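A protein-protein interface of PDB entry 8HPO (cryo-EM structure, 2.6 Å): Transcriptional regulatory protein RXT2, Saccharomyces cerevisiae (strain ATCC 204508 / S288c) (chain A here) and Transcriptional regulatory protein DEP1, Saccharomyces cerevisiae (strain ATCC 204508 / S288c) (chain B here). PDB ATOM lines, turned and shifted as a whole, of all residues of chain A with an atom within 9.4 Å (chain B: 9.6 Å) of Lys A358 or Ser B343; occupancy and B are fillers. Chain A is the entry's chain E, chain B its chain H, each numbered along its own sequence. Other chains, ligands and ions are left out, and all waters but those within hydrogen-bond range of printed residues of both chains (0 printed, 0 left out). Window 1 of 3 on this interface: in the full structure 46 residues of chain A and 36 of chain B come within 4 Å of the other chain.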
ATOM      1  N   LEU A 190       6.837  -7.882 -21.047  1.00  0.00           N
ATOM      2  CA  LEU A 190       7.830  -8.946 -21.088  1.00  0.00           C
ATOM      3  C   LEU A 190       7.762  -9.803 -19.832  1.00  0.00           C
ATOM      4  O   LEU A 190       8.399 -10.859 -19.758  1.00  0.00           O
ATOM      5  CB  LEU A 190       9.226  -8.359 -21.259  1.00  0.00           C
ATOM      6  CG  LEU A 190       9.504  -7.619 -22.560  1.00  0.00           C
ATOM      7  CD1 LEU A 190      10.898  -7.021 -22.529  1.00  0.00           C
ATOM      8  CD2 LEU A 190       9.337  -8.541 -23.750  1.00  0.00           C
ATOM      9  N   ALA A 194       6.637 -14.296 -19.752  1.00  0.00           N
ATOM     10  CA  ALA A 194       7.391 -15.286 -18.996  1.00  0.00           C
ATOM     11  C   ALA A 194       6.481 -16.081 -18.067  1.00  0.00           C
ATOM     12  O   ALA A 194       6.667 -17.291 -17.881  1.00  0.00           O
ATOM     13  CB  ALA A 194       8.505 -14.596 -18.215  1.00  0.00           C
ATOM     14  N   GLN A 350      11.872 -23.829 -22.671  1.00  0.00           N
ATOM     15  CA  GLN A 350      12.813 -23.237 -21.730  1.00  0.00           C
ATOM     16  C   GLN A 350      13.792 -22.307 -22.431  1.00  0.00           C
ATOM     17  O   GLN A 350      14.111 -21.229 -21.907  1.00  0.00           O
ATOM     18  CB  GLN A 350      13.554 -24.332 -20.974  1.00  0.00           C
ATOM     19  CG  GLN A 350      12.639 -25.180 -20.132  1.00  0.00           C
ATOM     20  CD  GLN A 350      13.352 -25.841 -18.985  1.00  0.00           C
ATOM     21  OE1 GLN A 350      14.579 -25.891 -18.952  1.00  0.00           O
ATOM     22  NE2 GLN A 350      12.588 -26.350 -18.031  1.00  0.00           N
ATOM     23  N   LYS A 351      14.280 -22.695 -23.612  1.00  0.00           N
ATOM     24  CA  LYS A 351      15.119 -21.768 -24.374  1.00  0.00           C
ATOM     25  C   LYS A 351      14.374 -20.463 -24.669  1.00  0.00           C
ATOM     26  O   LYS A 351      14.926 -19.356 -24.543  1.00  0.00           O
ATOM     27  CB  LYS A 351      15.584 -22.427 -25.671  1.00  0.00           C
ATOM     28  CG  LYS A 351      16.151 -23.825 -25.520  1.00  0.00           C
ATOM     29  CD  LYS A 351      17.658 -23.820 -25.653  1.00  0.00           C
ATOM     30  CE  LYS A 351      18.157 -25.008 -26.454  1.00  0.00           C
ATOM     31  NZ  LYS A 351      17.064 -25.864 -26.977  1.00  0.00           N
ATOM     32  N   ILE A 352      13.100 -20.581 -25.042  1.00  0.00           N
ATOM     33  CA  ILE A 352      12.290 -19.401 -25.343  1.00  0.00           C
ATOM     34  C   ILE A 352      12.205 -18.480 -24.128  1.00  0.00           C
ATOM     35  O   ILE A 352      12.499 -17.276 -24.214  1.00  0.00           O
ATOM     36  CB  ILE A 352      10.895 -19.828 -25.832  1.00  0.00           C
ATOM     37  CG1 ILE A 352      10.952 -20.235 -27.302  1.00  0.00           C
ATOM     38  CG2 ILE A 352       9.887 -18.723 -25.620  1.00  0.00           C
ATOM     39  CD1 ILE A 352       9.910 -21.230 -27.688  1.00  0.00           C
ATOM     40  N   ARG A 353      11.787 -19.030 -22.981  1.00  0.00           N
ATOM     41  CA  ARG A 353      11.638 -18.206 -21.782  1.00  0.00           C
ATOM     42  C   ARG A 353      12.952 -17.566 -21.370  1.00  0.00           C
ATOM     43  O   ARG A 353      12.961 -16.443 -20.848  1.00  0.00           O
ATOM     44  CB  ARG A 353      11.080 -19.032 -20.629  1.00  0.00           C
ATOM     45  CG  ARG A 353      10.762 -18.207 -19.398  1.00  0.00           C
ATOM     46  CD  ARG A 353      10.261 -19.055 -18.255  1.00  0.00           C
ATOM     47  NE  ARG A 353       9.527 -18.265 -17.273  1.00  0.00           N
ATOM     48  CZ  ARG A 353      10.096 -17.617 -16.265  1.00  0.00           C
ATOM     49  NH1 ARG A 353      11.407 -17.670 -16.103  1.00  0.00           N
ATOM     50  NH2 ARG A 353       9.359 -16.920 -15.419  1.00  0.00           N
ATOM     51  N   LYS A 354      14.071 -18.249 -21.606  1.00  0.00           N
ATOM     52  CA  LYS A 354      15.367 -17.649 -21.312  1.00  0.00           C
ATOM     53  C   LYS A 354      15.590 -16.390 -22.140  1.00  0.00           C
ATOM     54  O   LYS A 354      16.024 -15.354 -21.612  1.00  0.00           O
ATOM     55  CB  LYS A 354      16.466 -18.676 -21.561  1.00  0.00           C
ATOM     56  CG  LYS A 354      17.785 -18.113 -21.999  1.00  0.00           C
ATOM     57  CD  LYS A 354      18.850 -19.175 -21.882  1.00  0.00           C
ATOM     58  CE  LYS A 354      20.153 -18.720 -22.502  1.00  0.00           C
ATOM     59  NZ  LYS A 354      19.919 -18.006 -23.781  1.00  0.00           N
ATOM     60  N   SER A 355      15.261 -16.447 -23.431  1.00  0.00           N
ATOM     61  CA  SER A 355      15.406 -15.253 -24.265  1.00  0.00           C
ATOM     62  C   SER A 355      14.514 -14.113 -23.778  1.00  0.00           C
ATOM     63  O   SER A 355      14.941 -12.947 -23.720  1.00  0.00           O
ATOM     64  CB  SER A 355      15.086 -15.596 -25.715  1.00  0.00           C
ATOM     65  OG  SER A 355      16.225 -16.128 -26.366  1.00  0.00           O
ATOM     66  N   VAL A 356      13.272 -14.436 -23.413  1.00  0.00           N
ATOM     67  CA  VAL A 356      12.323 -13.401 -23.001  1.00  0.00           C
ATOM     68  C   VAL A 356      12.795 -12.694 -21.730  1.00  0.00           C
ATOM     69  O   VAL A 356      12.762 -11.456 -21.635  1.00  0.00           O
ATOM     70  CB  VAL A 356      10.922 -14.006 -22.825  1.00  0.00           C
ATOM     71  CG1 VAL A 356      10.017 -13.038 -22.109  1.00  0.00           C
ATOM     72  CG2 VAL A 356      10.340 -14.371 -24.169  1.00  0.00           C
ATOM     73  N   ILE A 357      13.247 -13.459 -20.734  1.00  0.00           N
ATOM     74  CA  ILE A 357      13.638 -12.804 -19.489  1.00  0.00           C
ATOM     75  C   ILE A 357      14.977 -12.090 -19.640  1.00  0.00           C
ATOM     76  O   ILE A 357      15.248 -11.119 -18.921  1.00  0.00           O
ATOM     77  CB  ILE A 357      13.654 -13.802 -18.318  1.00  0.00           C
ATOM     78  CG1 ILE A 357      14.819 -14.777 -18.446  1.00  0.00           C
ATOM     79  CG2 ILE A 357      12.333 -14.535 -18.223  1.00  0.00           C
ATOM     80  CD1 ILE A 357      14.730 -15.929 -17.509  1.00  0.00           C
ATOM     81  N   LYS A 358      15.809 -12.503 -20.598  1.00  0.00           N
ATOM     82  CA  LYS A 358      17.008 -11.730 -20.903  1.00  0.00           C
ATOM     83  C   LYS A 358      16.647 -10.344 -21.429  1.00  0.00           C
ATOM     84  O   LYS A 358      17.216  -9.322 -21.002  1.00  0.00           O
ATOM     85  CB  LYS A 358      17.847 -12.495 -21.921  1.00  0.00           C
ATOM     86  CG  LYS A 358      19.273 -12.059 -22.037  1.00  0.00           C
ATOM     87  CD  LYS A 358      19.930 -12.801 -23.176  1.00  0.00           C
ATOM     88  CE  LYS A 358      21.372 -13.127 -22.859  1.00  0.00           C
ATOM     89  NZ  LYS A 358      21.604 -14.590 -22.849  1.00  0.00           N
ATOM     90  N   ALA A 359      15.684 -10.292 -22.355  1.00  0.00           N
ATOM     91  CA  ALA A 359      15.222  -9.003 -22.868  1.00  0.00           C
ATOM     92  C   ALA A 359      14.658  -8.132 -21.752  1.00  0.00           C
ATOM     93  O   ALA A 359      14.961  -6.934 -21.668  1.00  0.00           O
ATOM     94  CB  ALA A 359      14.173  -9.213 -23.958  1.00  0.00           C
ATOM     95  N   ASN A 360      13.817  -8.718 -20.893  1.00  0.00           N
ATOM     96  CA  ASN A 360      13.210  -7.950 -19.806  1.00  0.00           C
ATOM     97  C   ASN A 360      14.260  -7.385 -18.851  1.00  0.00           C
ATOM     98  O   ASN A 360      14.139  -6.242 -18.386  1.00  0.00           O
ATOM     99  CB  ASN A 360      12.212  -8.817 -19.050  1.00  0.00           C
ATOM    100  CG  ASN A 360      11.466  -8.055 -17.989  1.00  0.00           C
ATOM    101  OD1 ASN A 360      11.068  -8.613 -16.972  1.00  0.00           O
ATOM    102  ND2 ASN A 360      11.258  -6.776 -18.224  1.00  0.00           N
ATOM    103  N   ARG A 361      15.304  -8.157 -18.552  1.00  0.00           N
ATOM    104  CA  ARG A 361      16.339  -7.646 -17.659  1.00  0.00           C
ATOM    105  C   ARG A 361      17.083  -6.472 -18.284  1.00  0.00           C
ATOM    106  O   ARG A 361      17.368  -5.477 -17.605  1.00  0.00           O
ATOM    107  CB  ARG A 361      17.313  -8.761 -17.282  1.00  0.00           C
ATOM    108  CG  ARG A 361      18.565  -8.276 -16.577  1.00  0.00           C
ATOM    109  CD  ARG A 361      19.227  -9.379 -15.785  1.00  0.00           C
ATOM    110  NE  ARG A 361      20.670  -9.420 -15.996  1.00  0.00           N
ATOM    111  CZ  ARG A 361      21.570  -9.143 -15.062  1.00  0.00           C
ATOM    112  NH1 ARG A 361      22.863  -9.203 -15.340  1.00  0.00           N
ATOM    113  NH2 ARG A 361      21.178  -8.797 -13.849  1.00  0.00           N
ATOM    114  N   ILE A 362      17.422  -6.573 -19.575  1.00  0.00           N
ATOM    115  CA  ILE A 362      18.116  -5.463 -20.232  1.00  0.00           C
ATOM    116  C   ILE A 362      17.251  -4.205 -20.210  1.00  0.00           C
ATOM    117  O   ILE A 362      17.731  -3.100 -19.901  1.00  0.00           O
ATOM    118  CB  ILE A 362      18.512  -5.859 -21.666  1.00  0.00           C
ATOM    119  CG1 ILE A 362      19.847  -6.595 -21.664  1.00  0.00           C
ATOM    120  CG2 ILE A 362      18.598  -4.646 -22.568  1.00  0.00           C
ATOM    121  CD1 ILE A 362      20.075  -7.429 -22.883  1.00  0.00           C
ATOM    122  N   ARG A 363      15.964  -4.359 -20.527  1.00  0.00           N
ATOM    123  CA  ARG A 363      15.014  -3.254 -20.428  1.00  0.00           C
ATOM    124  C   ARG A 363      15.070  -2.577 -19.064  1.00  0.00           C
ATOM    125  O   ARG A 363      15.175  -1.345 -18.978  1.00  0.00           O
ATOM    126  CB  ARG A 363      13.612  -3.778 -20.702  1.00  0.00           C
ATOM    127  CG  ARG A 363      12.500  -2.831 -20.385  1.00  0.00           C
ATOM    128  CD  ARG A 363      11.228  -3.614 -20.203  1.00  0.00           C
ATOM    129  NE  ARG A 363      10.396  -3.098 -19.123  1.00  0.00           N
ATOM    130  CZ  ARG A 363      10.708  -3.146 -17.831  1.00  0.00           C
ATOM    131  NH1 ARG A 363      11.841  -3.694 -17.425  1.00  0.00           N
ATOM    132  NH2 ARG A 363       9.871  -2.645 -16.940  1.00  0.00           N
ATOM    133  N   GLY A 364      14.979  -3.365 -17.988  1.00  0.00           N
ATOM    134  CA  GLY A 364      14.970  -2.787 -16.652  1.00  0.00           C
ATOM    135  C   GLY A 364      16.259  -2.070 -16.291  1.00  0.00           C
ATOM    136  O   GLY A 364      16.233  -1.028 -15.630  1.00  0.00           O
ATOM    137  N   ARG A 365      17.404  -2.610 -16.714  1.00  0.00           N
ATOM    138  CA  ARG A 365      18.654  -1.911 -16.428  1.00  0.00           C
ATOM    139  C   ARG A 365      18.708  -0.565 -17.139  1.00  0.00           C
ATOM    140  O   ARG A 365      19.201   0.423 -16.574  1.00  0.00           O
ATOM    141  CB  ARG A 365      19.869  -2.751 -16.820  1.00  0.00           C
ATOM    142  CG  ARG A 365      19.816  -4.206 -16.431  1.00  0.00           C
ATOM    143  CD  ARG A 365      20.019  -4.413 -14.950  1.00  0.00           C
ATOM    144  NE  ARG A 365      21.332  -3.969 -14.491  1.00  0.00           N
ATOM    145  CZ  ARG A 365      22.480  -4.555 -14.810  1.00  0.00           C
ATOM    146  NH1 ARG A 365      23.622  -4.077 -14.339  1.00  0.00           N
ATOM    147  NH2 ARG A 365      22.491  -5.613 -15.601  1.00  0.00           N
ATOM    148  N   ILE A 366      18.206  -0.497 -18.375  1.00  0.00           N
ATOM    149  CA  ILE A 366      18.206   0.789 -19.068  1.00  0.00           C
ATOM    150  C   ILE A 366      17.283   1.771 -18.360  1.00  0.00           C
ATOM    151  O   ILE A 366      17.630   2.941 -18.163  1.00  0.00           O
ATOM    152  CB  ILE A 366      17.821   0.628 -20.550  1.00  0.00           C
ATOM    153  CG1 ILE A 366      18.738  -0.371 -21.248  1.00  0.00           C
ATOM    154  CG2 ILE A 366      17.913   1.966 -21.259  1.00  0.00           C
ATOM    155  CD1 ILE A 366      20.120   0.151 -21.492  1.00  0.00           C
ATOM    156  N   TRP A 369      19.146   3.102 -15.192  1.00  0.00           N
ATOM    157  CA  TRP A 369      20.206   4.062 -15.478  1.00  0.00           C
ATOM    158  C   TRP A 369      19.635   5.382 -15.978  1.00  0.00           C
ATOM    159  O   TRP A 369      20.177   6.454 -15.681  1.00  0.00           O
ATOM    160  CB  TRP A 369      21.176   3.488 -16.499  1.00  0.00           C
ATOM    161  CG  TRP A 369      22.061   2.456 -15.938  1.00  0.00           C
ATOM    162  CD1 TRP A 369      22.466   2.341 -14.648  1.00  0.00           C
ATOM    163  CD2 TRP A 369      22.660   1.376 -16.649  1.00  0.00           C
ATOM    164  NE1 TRP A 369      23.288   1.254 -14.507  1.00  0.00           N
ATOM    165  CE2 TRP A 369      23.424   0.645 -15.726  1.00  0.00           C
ATOM    166  CE3 TRP A 369      22.629   0.958 -17.981  1.00  0.00           C
ATOM    167  CZ2 TRP A 369      24.143  -0.485 -16.089  1.00  0.00           C
ATOM    168  CZ3 TRP A 369      23.349  -0.157 -18.339  1.00  0.00           C
ATOM    169  CH2 TRP A 369      24.097  -0.866 -17.399  1.00  0.00           C
ATOM    170  N   VAL B 335      37.111 -11.761 -20.954  1.00  0.00           N
ATOM    171  CA  VAL B 335      35.950 -10.886 -20.877  1.00  0.00           C
ATOM    172  C   VAL B 335      36.053 -10.095 -19.582  1.00  0.00           C
ATOM    173  O   VAL B 335      36.545 -10.609 -18.570  1.00  0.00           O
ATOM    174  CB  VAL B 335      34.635 -11.692 -20.936  1.00  0.00           C
ATOM    175  CG1 VAL B 335      33.436 -10.774 -21.010  1.00  0.00           C
ATOM    176  CG2 VAL B 335      34.649 -12.622 -22.121  1.00  0.00           C
ATOM    177  N   ALA B 336      35.605  -8.846 -19.612  1.00  0.00           N
ATOM    178  CA  ALA B 336      35.557  -8.062 -18.389  1.00  0.00           C
ATOM    179  C   ALA B 336      34.402  -8.535 -17.519  1.00  0.00           C
ATOM    180  O   ALA B 336      33.360  -8.965 -18.021  1.00  0.00           O
ATOM    181  CB  ALA B 336      35.412  -6.577 -18.712  1.00  0.00           C
ATOM    182  N   GLU B 337      34.589  -8.442 -16.201  1.00  0.00           N
ATOM    183  CA  GLU B 337      33.652  -9.066 -15.273  1.00  0.00           C
ATOM    184  C   GLU B 337      32.308  -8.353 -15.267  1.00  0.00           C
ATOM    185  O   GLU B 337      31.256  -8.993 -15.146  1.00  0.00           O
ATOM    186  CB  GLU B 337      34.260  -9.090 -13.875  1.00  0.00           C
ATOM    187  CG  GLU B 337      35.766  -9.266 -13.881  1.00  0.00           C
ATOM    188  CD  GLU B 337      36.296  -9.739 -12.549  1.00  0.00           C
ATOM    189  OE1 GLU B 337      35.515  -9.761 -11.578  1.00  0.00           O
ATOM    190  OE2 GLU B 337      37.488 -10.097 -12.472  1.00  0.00           O
ATOM    191  N   ASP B 338      32.321  -7.026 -15.385  1.00  0.00           N
ATOM    192  CA  ASP B 338      31.076  -6.273 -15.486  1.00  0.00           C
ATOM    193  C   ASP B 338      30.249  -6.743 -16.675  1.00  0.00           C
ATOM    194  O   ASP B 338      29.027  -6.925 -16.574  1.00  0.00           O
ATOM    195  CB  ASP B 338      31.396  -4.784 -15.595  1.00  0.00           C
ATOM    196  CG  ASP B 338      32.598  -4.513 -16.474  1.00  0.00           C
ATOM    197  OD1 ASP B 338      33.678  -4.208 -15.934  1.00  0.00           O
ATOM    198  OD2 ASP B 338      32.462  -4.603 -17.707  1.00  0.00           O
ATOM    199  N   LEU B 339      30.907  -6.945 -17.818  1.00  0.00           N
ATOM    200  CA  LEU B 339      30.222  -7.494 -18.978  1.00  0.00           C
ATOM    201  C   LEU B 339      29.707  -8.896 -18.701  1.00  0.00           C
ATOM    202  O   LEU B 339      28.612  -9.248 -19.141  1.00  0.00           O
ATOM    203  CB  LEU B 339      31.152  -7.491 -20.191  1.00  0.00           C
ATOM    204  CG  LEU B 339      31.940  -6.200 -20.408  1.00  0.00           C
ATOM    205  CD1 LEU B 339      32.957  -6.356 -21.518  1.00  0.00           C
ATOM    206  CD2 LEU B 339      30.995  -5.055 -20.713  1.00  0.00           C
ATOM    207  N   ALA B 340      30.474  -9.708 -17.973  1.00  0.00           N
ATOM    208  CA  ALA B 340      30.000 -11.035 -17.610  1.00  0.00           C
ATOM    209  C   ALA B 340      28.776 -10.982 -16.705  1.00  0.00           C
ATOM    210  O   ALA B 340      28.014 -11.950 -16.661  1.00  0.00           O
ATOM    211  CB  ALA B 340      31.120 -11.825 -16.940  1.00  0.00           C
ATOM    212  N   CYS B 341      28.565  -9.877 -15.989  1.00  0.00           N
ATOM    213  CA  CYS B 341      27.322  -9.718 -15.240  1.00  0.00           C
ATOM    214  C   CYS B 341      26.170  -9.244 -16.119  1.00  0.00           C
ATOM    215  O   CYS B 341      25.062  -9.776 -16.003  1.00  0.00           O
ATOM    216  CB  CYS B 341      27.521  -8.756 -14.068  1.00  0.00           C
ATOM    217  SG  CYS B 341      28.963  -9.114 -13.044  1.00  0.00           S
ATOM    218  N   GLU B 342      26.387  -8.245 -16.981  1.00  0.00           N
ATOM    219  CA  GLU B 342      25.375  -7.865 -17.977  1.00  0.00           C
ATOM    220  C   GLU B 342      25.342  -9.002 -18.979  1.00  0.00           C
ATOM    221  O   GLU B 342      26.126  -9.024 -19.922  1.00  0.00           O
ATOM    222  CB  GLU B 342      25.717  -6.544 -18.650  1.00  0.00           C
ATOM    223  CG  GLU B 342      26.109  -5.433 -17.708  1.00  0.00           C
ATOM    224  CD  GLU B 342      24.918  -4.713 -17.137  1.00  0.00           C
ATOM    225  OE1 GLU B 342      23.780  -5.044 -17.527  1.00  0.00           O
ATOM    226  OE2 GLU B 342      25.116  -3.817 -16.295  1.00  0.00           O
ATOM    227  N   SER B 343      24.345  -9.885 -18.858  1.00  0.00           N
ATOM    228  CA  SER B 343      24.668 -11.306 -18.789  1.00  0.00           C
ATOM    229  C   SER B 343      25.837 -11.695 -19.687  1.00  0.00           C
ATOM    230  O   SER B 343      26.922 -11.915 -19.143  1.00  0.00           O
ATOM    231  CB  SER B 343      23.444 -12.144 -19.143  1.00  0.00           C
ATOM    232  OG  SER B 343      23.359 -12.325 -20.541  1.00  0.00           O
ATOM    233  N   ILE B 344      25.658 -11.875 -21.005  1.00  0.00           N
ATOM    234  CA  ILE B 344      26.552 -11.357 -22.052  1.00  0.00           C
ATOM    235  C   ILE B 344      26.286 -12.103 -23.358  1.00  0.00           C
ATOM    236  O   ILE B 344      25.645 -13.161 -23.353  1.00  0.00           O
ATOM    237  CB  ILE B 344      28.048 -11.392 -21.680  1.00  0.00           C
ATOM    238  CG1 ILE B 344      28.826 -10.372 -22.520  1.00  0.00           C
ATOM    239  CG2 ILE B 344      28.622 -12.789 -21.831  1.00  0.00           C
ATOM    240  CD1 ILE B 344      28.131  -9.019 -22.661  1.00  0.00           C
ATOM    241  N   GLU B 345      26.736 -11.550 -24.485  1.00  0.00           N
ATOM    242  CA  GLU B 345      27.495 -12.328 -25.469  1.00  0.00           C
ATOM    243  C   GLU B 345      28.311 -11.352 -26.305  1.00  0.00           C
ATOM    244  O   GLU B 345      27.782 -10.715 -27.220  1.00  0.00           O
ATOM    245  CB  GLU B 345      26.622 -13.217 -26.352  1.00  0.00           C
ATOM    246  CG  GLU B 345      27.449 -14.379 -26.903  1.00  0.00           C
ATOM    247  CD  GLU B 345      26.964 -14.924 -28.225  1.00  0.00           C
ATOM    248  OE1 GLU B 345      26.196 -14.228 -28.919  1.00  0.00           O
ATOM    249  OE2 GLU B 345      27.373 -16.051 -28.576  1.00  0.00           O
ATOM    250  N   TYR B 346      29.601 -11.267 -26.010  1.00  0.00           N
ATOM    251  CA  TYR B 346      30.455 -10.168 -26.442  1.00  0.00           C
ATOM    252  C   TYR B 346      31.279 -10.587 -27.656  1.00  0.00           C
ATOM    253  O   TYR B 346      31.979 -11.604 -27.616  1.00  0.00           O
ATOM    254  CB  TYR B 346      31.358  -9.753 -25.282  1.00  0.00           C
ATOM    255  CG  TYR B 346      32.135  -8.468 -25.446  1.00  0.00           C
ATOM    256  CD1 TYR B 346      33.499  -8.492 -25.704  1.00  0.00           C
ATOM    257  CD2 TYR B 346      31.522  -7.235 -25.290  1.00  0.00           C
ATOM    258  CE1 TYR B 346      34.224  -7.324 -25.833  1.00  0.00           C
ATOM    259  CE2 TYR B 346      32.238  -6.061 -25.420  1.00  0.00           C
ATOM    260  CZ  TYR B 346      33.592  -6.113 -25.691  1.00  0.00           C
ATOM    261  OH  TYR B 346      34.315  -4.952 -25.817  1.00  0.00           O
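OE2 of Glu B342 lies within salt-bridge range of NH1 of Arg A365 (2.5 Å).
NH1 of Arg A361 sits close to O of Cys B341 (2.4 Å).
Among the printed residues, pairs that only touch across the chains: Lys A358 with Ser B343, Arg A361 with Glu B342, Arg A361 with Ser B343 and Trp A369 with Glu B342.
Of the 12 printed residues of chain B, 3 touch a printed residue of chain A.
Among the printed residues, 6 pairs touch across the chains.
Among the printed residues, Asp or Glu carboxylates within 4 Å of a Lys or Arg side-chain nitrogen of the other chain: Arg A365 with Glu B342 (2.4 Å).
SG of Cys B341 sits at hydrogen-bond distance from O of Glu B337 (3.1 Å).
Lys A358 touches just one residue of chain B: Ser B343 (3.2 Å).
Of chain A, only Lys A358 (3.2 Å) and Arg A361 (3.9 Å) come within 4 Å of Ser B343.
No residue of chain B comes within 4 Å of Ala A359.
No residue of chain A comes within 4 Å of Ala B340.
Of the printed residues of chain B, Trp A369 touches Glu B342 (3.3 Å).
Of the printed residues of chain B, Arg A361 touches Cys B341 (2.4 Å), Glu B342 (3.9 Å) and Ser B343 (3.9 Å).
Printed residues of chain A within 4 Å of Glu B342: Arg A361, Arg A365 and Trp A369.
Of the printed residues of chain B, Arg A365 touches Glu B342.
Printed residues of chain A within 4 Å of Cys B341: Arg A361.
Gln A350 touches none of the printed residues of chain B.
The nearest residue of chain A that does not touch Ser B343 is Arg A365 (5.7 Å).
The nearest printed residue of chain B that does not touch Arg A365 is Cys B341 (4.9 Å).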
